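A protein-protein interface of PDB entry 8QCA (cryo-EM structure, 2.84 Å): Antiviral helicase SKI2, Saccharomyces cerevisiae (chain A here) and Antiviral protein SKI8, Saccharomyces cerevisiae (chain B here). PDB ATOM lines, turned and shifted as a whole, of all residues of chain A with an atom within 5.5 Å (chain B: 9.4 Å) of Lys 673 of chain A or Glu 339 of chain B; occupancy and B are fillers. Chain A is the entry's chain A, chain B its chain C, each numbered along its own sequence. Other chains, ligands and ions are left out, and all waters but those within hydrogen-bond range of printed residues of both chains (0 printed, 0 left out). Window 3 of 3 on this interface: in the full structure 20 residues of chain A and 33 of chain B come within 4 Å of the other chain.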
ATOM      1  N   LEU A 671       4.313  10.163 -12.920  1.00  0.00           N
ATOM      2  CA  LEU A 671       4.127  11.590 -13.129  1.00  0.00           C
ATOM      3  C   LEU A 671       5.273  12.372 -12.498  1.00  0.00           C
ATOM      4  O   LEU A 671       6.124  11.826 -11.793  1.00  0.00           O
ATOM      5  CB  LEU A 671       2.788  12.044 -12.542  1.00  0.00           C
ATOM      6  CG  LEU A 671       1.530  11.317 -13.021  1.00  0.00           C
ATOM      7  CD1 LEU A 671       0.321  11.767 -12.220  1.00  0.00           C
ATOM      8  CD2 LEU A 671       1.309  11.543 -14.505  1.00  0.00           C
ATOM      9  N   LYS A 672       5.287  13.673 -12.762  1.00  0.00           N
ATOM     10  CA  LYS A 672       6.245  14.569 -12.138  1.00  0.00           C
ATOM     11  C   LYS A 672       5.717  15.054 -10.792  1.00  0.00           C
ATOM     12  O   LYS A 672       4.558  14.840 -10.435  1.00  0.00           O
ATOM     13  CB  LYS A 672       6.541  15.763 -13.041  1.00  0.00           C
ATOM     14  CG  LYS A 672       7.276  15.425 -14.316  1.00  0.00           C
ATOM     15  CD  LYS A 672       7.743  16.691 -15.002  1.00  0.00           C
ATOM     16  CE  LYS A 672       6.570  17.507 -15.509  1.00  0.00           C
ATOM     17  NZ  LYS A 672       7.027  18.730 -16.222  1.00  0.00           N
ATOM     18  N   LYS A 673       6.589  15.726 -10.040  1.00  0.00           N
ATOM     19  CA  LYS A 673       6.168  16.307  -8.771  1.00  0.00           C
ATOM     20  C   LYS A 673       5.125  17.398  -8.977  1.00  0.00           C
ATOM     21  O   LYS A 673       4.233  17.567  -8.137  1.00  0.00           O
ATOM     22  CB  LYS A 673       7.379  16.856  -8.017  1.00  0.00           C
ATOM     23  CG  LYS A 673       7.054  17.406  -6.641  1.00  0.00           C
ATOM     24  CD  LYS A 673       8.306  17.872  -5.922  1.00  0.00           C
ATOM     25  CE  LYS A 673       7.957  18.648  -4.662  1.00  0.00           C
ATOM     26  NZ  LYS A 673       7.262  17.794  -3.661  1.00  0.00           N
ATOM     27  N   GLU A 674       5.219  18.147 -10.078  1.00  0.00           N
ATOM     28  CA  GLU A 674       4.193  19.138 -10.387  1.00  0.00           C
ATOM     29  C   GLU A 674       2.856  18.472 -10.682  1.00  0.00           C
ATOM     30  O   GLU A 674       1.801  18.986 -10.294  1.00  0.00           O
ATOM     31  CB  GLU A 674       4.632  20.000 -11.570  1.00  0.00           C
ATOM     32  CG  GLU A 674       6.112  20.328 -11.589  1.00  0.00           C
ATOM     33  CD  GLU A 674       6.456  21.398 -12.608  1.00  0.00           C
ATOM     34  OE1 GLU A 674       5.824  21.420 -13.685  1.00  0.00           O
ATOM     35  OE2 GLU A 674       7.359  22.216 -12.333  1.00  0.00           O
ATOM     36  N   ASP A 675       2.878  17.332 -11.377  1.00  0.00           N
ATOM     37  CA  ASP A 675       1.638  16.625 -11.676  1.00  0.00           C
ATOM     38  C   ASP A 675       1.083  15.931 -10.438  1.00  0.00           C
ATOM     39  O   ASP A 675      -0.137  15.879 -10.246  1.00  0.00           O
ATOM     40  CB  ASP A 675       1.867  15.616 -12.800  1.00  0.00           C
ATOM     41  CG  ASP A 675       2.262  16.278 -14.105  1.00  0.00           C
ATOM     42  OD1 ASP A 675       1.957  17.475 -14.283  1.00  0.00           O
ATOM     43  OD2 ASP A 675       2.878  15.601 -14.955  1.00  0.00           O
ATOM     44  N   ARG A 676       1.959  15.392  -9.587  1.00  0.00           N
ATOM     45  CA  ARG A 676       1.512  14.728  -8.369  1.00  0.00           C
ATOM     46  C   ARG A 676       0.846  15.687  -7.393  1.00  0.00           C
ATOM     47  O   ARG A 676       0.096  15.240  -6.519  1.00  0.00           O
ATOM     48  CB  ARG A 676       2.687  14.044  -7.669  1.00  0.00           C
ATOM     49  CG  ARG A 676       3.249  12.830  -8.384  1.00  0.00           C
ATOM     50  CD  ARG A 676       4.502  12.342  -7.677  1.00  0.00           C
ATOM     51  NE  ARG A 676       5.410  11.636  -8.572  1.00  0.00           N
ATOM     52  CZ  ARG A 676       6.722  11.825  -8.604  1.00  0.00           C
ATOM     53  NH1 ARG A 676       7.314  12.702  -7.812  1.00  0.00           N
ATOM     54  NH2 ARG A 676       7.458  11.117  -9.456  1.00  0.00           N
ATOM     55  N   ASP A 677       1.105  16.986  -7.516  1.00  0.00           N
ATOM     56  CA  ASP A 677       0.627  17.980  -6.566  1.00  0.00           C
ATOM     57  C   ASP A 677      -0.603  18.729  -7.058  1.00  0.00           C
ATOM     58  O   ASP A 677      -0.954  19.764  -6.485  1.00  0.00           O
ATOM     59  CB  ASP A 677       1.746  18.970  -6.240  1.00  0.00           C
ATOM     60  CG  ASP A 677       2.840  18.353  -5.391  1.00  0.00           C
ATOM     61  OD1 ASP A 677       2.541  17.410  -4.628  1.00  0.00           O
ATOM     62  OD2 ASP A 677       3.999  18.811  -5.486  1.00  0.00           O
ATOM     63  N   ASN B  10      13.728   5.032  -9.773  1.00  0.00           N
ATOM     64  CA  ASN B  10      14.768   6.016 -10.038  1.00  0.00           C
ATOM     65  C   ASN B  10      15.502   6.296  -8.737  1.00  0.00           C
ATOM     66  O   ASN B  10      15.030   5.961  -7.650  1.00  0.00           O
ATOM     67  CB  ASN B  10      14.190   7.303 -10.638  1.00  0.00           C
ATOM     68  CG  ASN B  10      12.956   7.790  -9.905  1.00  0.00           C
ATOM     69  OD1 ASN B  10      13.010   8.116  -8.720  1.00  0.00           O
ATOM     70  ND2 ASN B  10      11.835   7.847 -10.611  1.00  0.00           N
ATOM     71  N   GLY B  12      17.741   9.649  -7.487  1.00  0.00           N
ATOM     72  CA  GLY B  12      18.422  10.914  -7.658  1.00  0.00           C
ATOM     73  C   GLY B  12      19.572  11.073  -6.683  1.00  0.00           C
ATOM     74  O   GLY B  12      19.576  10.510  -5.589  1.00  0.00           O
ATOM     75  N   LYS B  13      20.564  11.863  -7.099  1.00  0.00           N
ATOM     76  CA  LYS B  13      21.787  12.068  -6.324  1.00  0.00           C
ATOM     77  C   LYS B  13      22.439  10.733  -5.969  1.00  0.00           C
ATOM     78  O   LYS B  13      22.931  10.531  -4.858  1.00  0.00           O
ATOM     79  CB  LYS B  13      21.513  12.896  -5.068  1.00  0.00           C
ATOM     80  N   HIS B 332      13.120  15.198 -16.855  1.00  0.00           N
ATOM     81  CA  HIS B 332      12.980  16.343 -15.967  1.00  0.00           C
ATOM     82  C   HIS B 332      13.600  16.017 -14.618  1.00  0.00           C
ATOM     83  O   HIS B 332      13.635  14.859 -14.197  1.00  0.00           O
ATOM     84  CB  HIS B 332      11.510  16.742 -15.780  1.00  0.00           C
ATOM     85  CG  HIS B 332      10.737  16.824 -17.060  1.00  0.00           C
ATOM     86  ND1 HIS B 332       9.899  15.817 -17.489  1.00  0.00           N
ATOM     87  CD2 HIS B 332      10.672  17.794 -18.003  1.00  0.00           C
ATOM     88  CE1 HIS B 332       9.354  16.163 -18.642  1.00  0.00           C
ATOM     89  NE2 HIS B 332       9.806  17.357 -18.976  1.00  0.00           N
ATOM     90  N   CYS B 333      14.095  17.055 -13.941  1.00  0.00           N
ATOM     91  CA  CYS B 333      14.683  16.866 -12.621  1.00  0.00           C
ATOM     92  C   CYS B 333      13.633  16.593 -11.553  1.00  0.00           C
ATOM     93  O   CYS B 333      13.981  16.103 -10.474  1.00  0.00           O
ATOM     94  CB  CYS B 333      15.514  18.090 -12.234  1.00  0.00           C
ATOM     95  SG  CYS B 333      14.563  19.606 -11.996  1.00  0.00           S
ATOM     96  N   ASP B 334      12.365  16.887 -11.828  1.00  0.00           N
ATOM     97  CA  ASP B 334      11.285  16.675 -10.874  1.00  0.00           C
ATOM     98  C   ASP B 334      10.670  15.286 -10.973  1.00  0.00           C
ATOM     99  O   ASP B 334       9.712  14.997 -10.250  1.00  0.00           O
ATOM    100  CB  ASP B 334      10.197  17.732 -11.071  1.00  0.00           C
ATOM    101  CG  ASP B 334      10.762  19.129 -11.204  1.00  0.00           C
ATOM    102  OD1 ASP B 334      11.185  19.701 -10.177  1.00  0.00           O
ATOM    103  OD2 ASP B 334      10.790  19.654 -12.336  1.00  0.00           O
ATOM    104  N   ASP B 335      11.191  14.425 -11.845  1.00  0.00           N
ATOM    105  CA  ASP B 335      10.695  13.062 -11.964  1.00  0.00           C
ATOM    106  C   ASP B 335      11.151  12.161 -10.824  1.00  0.00           C
ATOM    107  O   ASP B 335      10.652  11.037 -10.709  1.00  0.00           O
ATOM    108  CB  ASP B 335      11.140  12.460 -13.298  1.00  0.00           C
ATOM    109  CG  ASP B 335      10.174  12.762 -14.423  1.00  0.00           C
ATOM    110  OD1 ASP B 335       8.966  12.493 -14.261  1.00  0.00           O
ATOM    111  OD2 ASP B 335      10.625  13.267 -15.472  1.00  0.00           O
ATOM    112  N   ILE B 336      12.080  12.621  -9.986  1.00  0.00           N
ATOM    113  CA  ILE B 336      12.573  11.808  -8.882  1.00  0.00           C
ATOM    114  C   ILE B 336      11.471  11.639  -7.846  1.00  0.00           C
ATOM    115  O   ILE B 336      10.818  12.611  -7.445  1.00  0.00           O
ATOM    116  CB  ILE B 336      13.830  12.444  -8.269  1.00  0.00           C
ATOM    117  CG1 ILE B 336      14.927  12.578  -9.327  1.00  0.00           C
ATOM    118  CG2 ILE B 336      14.332  11.622  -7.094  1.00  0.00           C
ATOM    119  CD1 ILE B 336      15.190  11.307 -10.102  1.00  0.00           C
ATOM    120  N   GLU B 337      11.256  10.395  -7.411  1.00  0.00           N
ATOM    121  CA  GLU B 337      10.190  10.105  -6.457  1.00  0.00           C
ATOM    122  C   GLU B 337      10.423  10.819  -5.131  1.00  0.00           C
ATOM    123  O   GLU B 337       9.610  11.647  -4.706  1.00  0.00           O
ATOM    124  CB  GLU B 337      10.075   8.596  -6.246  1.00  0.00           C
ATOM    125  CG  GLU B 337       9.144   7.905  -7.224  1.00  0.00           C
ATOM    126  CD  GLU B 337       9.379   6.410  -7.294  1.00  0.00           C
ATOM    127  OE1 GLU B 337       9.618   5.794  -6.235  1.00  0.00           O
ATOM    128  OE2 GLU B 337       9.323   5.849  -8.409  1.00  0.00           O
ATOM    129  N   ILE B 338      11.531  10.511  -4.461  1.00  0.00           N
ATOM    130  CA  ILE B 338      11.853  11.150  -3.189  1.00  0.00           C
ATOM    131  C   ILE B 338      12.251  12.596  -3.474  1.00  0.00           C
ATOM    132  O   ILE B 338      13.261  12.852  -4.135  1.00  0.00           O
ATOM    133  CB  ILE B 338      12.960  10.402  -2.437  1.00  0.00           C
ATOM    134  CG1 ILE B 338      12.512   8.983  -2.070  1.00  0.00           C
ATOM    135  CG2 ILE B 338      13.361  11.163  -1.189  1.00  0.00           C
ATOM    136  CD1 ILE B 338      12.798   7.936  -3.123  1.00  0.00           C
ATOM    137  N   GLU B 339      11.455  13.543  -2.974  1.00  0.00           N
ATOM    138  CA  GLU B 339      11.675  14.953  -3.275  1.00  0.00           C
ATOM    139  C   GLU B 339      12.962  15.492  -2.666  1.00  0.00           C
ATOM    140  O   GLU B 339      13.486  16.500  -3.152  1.00  0.00           O
ATOM    141  CB  GLU B 339      10.487  15.784  -2.789  1.00  0.00           C
ATOM    142  N   GLU B 340      13.482  14.853  -1.618  1.00  0.00           N
ATOM    143  CA  GLU B 340      14.733  15.300  -1.018  1.00  0.00           C
ATOM    144  C   GLU B 340      15.945  14.978  -1.879  1.00  0.00           C
ATOM    145  O   GLU B 340      17.033  15.494  -1.602  1.00  0.00           O
ATOM    146  CB  GLU B 340      14.902  14.675   0.368  1.00  0.00           C
ATOM    147  N   ASP B 341      15.788  14.149  -2.909  1.00  0.00           N
ATOM    148  CA  ASP B 341      16.879  13.770  -3.794  1.00  0.00           C
ATOM    149  C   ASP B 341      16.881  14.559  -5.098  1.00  0.00           C
ATOM    150  O   ASP B 341      17.676  14.254  -5.991  1.00  0.00           O
ATOM    151  CB  ASP B 341      16.812  12.272  -4.091  1.00  0.00           C
ATOM    152  CG  ASP B 341      17.351  11.429  -2.957  1.00  0.00           C
ATOM    153  OD1 ASP B 341      18.043  11.981  -2.077  1.00  0.00           O
ATOM    154  OD2 ASP B 341      17.081  10.210  -2.941  1.00  0.00           O
ATOM    155  N   ILE B 342      16.017  15.559  -5.226  1.00  0.00           N
ATOM    156  CA  ILE B 342      15.909  16.326  -6.462  1.00  0.00           C
ATOM    157  C   ILE B 342      17.016  17.371  -6.501  1.00  0.00           C
ATOM    158  O   ILE B 342      17.197  18.139  -5.550  1.00  0.00           O
ATOM    159  CB  ILE B 342      14.523  16.978  -6.579  1.00  0.00           C
ATOM    160  CG1 ILE B 342      13.441  15.905  -6.718  1.00  0.00           C
ATOM    161  CG2 ILE B 342      14.477  17.934  -7.758  1.00  0.00           C
ATOM    162  CD1 ILE B 342      12.044  16.456  -6.889  1.00  0.00           C
ATOM    163  N   LEU B 343      17.762  17.397  -7.601  1.00  0.00           N
ATOM    164  CA  LEU B 343      18.843  18.356  -7.814  1.00  0.00           C
ATOM    165  C   LEU B 343      18.380  19.339  -8.883  1.00  0.00           C
ATOM    166  O   LEU B 343      18.513  19.075 -10.081  1.00  0.00           O
ATOM    167  CB  LEU B 343      20.130  17.644  -8.224  1.00  0.00           C
ATOM    168  CG  LEU B 343      21.372  18.518  -8.397  1.00  0.00           C
ATOM    169  CD1 LEU B 343      21.763  19.151  -7.074  1.00  0.00           C
ATOM    170  CD2 LEU B 343      22.524  17.713  -8.970  1.00  0.00           C
ATOM    171  N   ALA B 344      17.830  20.474  -8.446  1.00  0.00           N
ATOM    172  CA  ALA B 344      17.294  21.452  -9.387  1.00  0.00           C
ATOM    173  C   ALA B 344      18.398  22.240 -10.084  1.00  0.00           C
ATOM    174  O   ALA B 344      18.298  22.523 -11.283  1.00  0.00           O
ATOM    175  CB  ALA B 344      16.335  22.400  -8.667  1.00  0.00           C
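The side-chain sulfur (SG) of Cys 333 of chain B sits at hydrogen-bond distance from the side-chain carboxylate (OD2) of Asp 334 of chain B, at 3.8 Å. A ring nitrogen (ND1) of His 332 of chain B sits at hydrogen-bond distance from the side-chain carboxylate (OD2) of Asp 335 of chain B, 3.3 Å away. NZ of Lys 673 of chain A lies within salt-bridge range of OD2 of Asp 677 of chain A (3.9 Å). The backbone carbonyl oxygen (O) of Leu 671 of chain A sits at hydrogen-bond distance from the guanidinium group (NH2) of Arg 676 of chain A, 2.8 Å away. The side-chain amino group (NZ) of Lys 672 of chain A is in salt-bridge range of the side-chain carboxylate (OE1) of Glu 674 of chain A (3.9 Å). The side-chain amide nitrogen of Asn 10 of chain B is in hydrogen-bond range of the backbone carbonyl oxygen of Asp 335 of chain B, 3.4 Å away.
Among the printed residues, merely in contact across the chains: Leu 671 of chain A with Asp 335 of chain B (3.8 Å), Lys 672 of chain A with His 332 of chain B (3.4 Å), Lys 672 of chain A with Asp 334 of chain B (3.97 Å), Lys 672 of chain A with Asp 335 of chain B (3.4 Å), Lys 673 of chain A with Glu 339 of chain B (3.9 Å) and Arg 676 of chain A with Ile 336 of chain B (3.5 Å).
Of chain B, only Asp 334 and Glu 339 come within 4 Å of Lys 673 of chain A. Glu 674 of chain A touches none of the printed residues of chain B. Printed residues of chain A within 4 Å of Asp 335 of chain B: Leu 671, Lys 672 and Arg 676. Of the printed residues of chain A, Ile 336 of chain B touches Arg 676 (3.5 Å). Glu 339 of chain B touches one residue of chain A. Glu 340 of chain B touches none of the printed residues of chain A. The nearest residue of chain B that does not touch Lys 673 of chain A is Ile 342 of chain B (4.1 Å). The nearest printed residue of chain A that does not touch Glu 339 of chain B is Arg 676 of chain A (6.4 Å). The nearest printed residue of chain A that does not touch Ile 336 of chain B is Lys 673 of chain A (5.5 Å).
Of the 16 printed residues of chain B, 5 touch a printed residue of chain A. Hydrophobic or aromatic side chains of chain B within 4 Å of the printed part of chain A: His 332. Of the 7 printed residues of chain A, 4 touch a printed residue of chain B. Among the printed residues, 8 pairs touch across the chains. Among the printed residues, no Asp or Glu carboxylate lies within 4 Å of a Lys or Arg side-chain nitrogen of the other chain.
N of Lys 673 of chain A is in hydrogen-bond range of O of Asp 334 of chain B, 3.2 Å away. O of Asp 335 of chain B is in hydrogen-bond range of NH2 of Arg 676 of chain A (3.4 Å).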
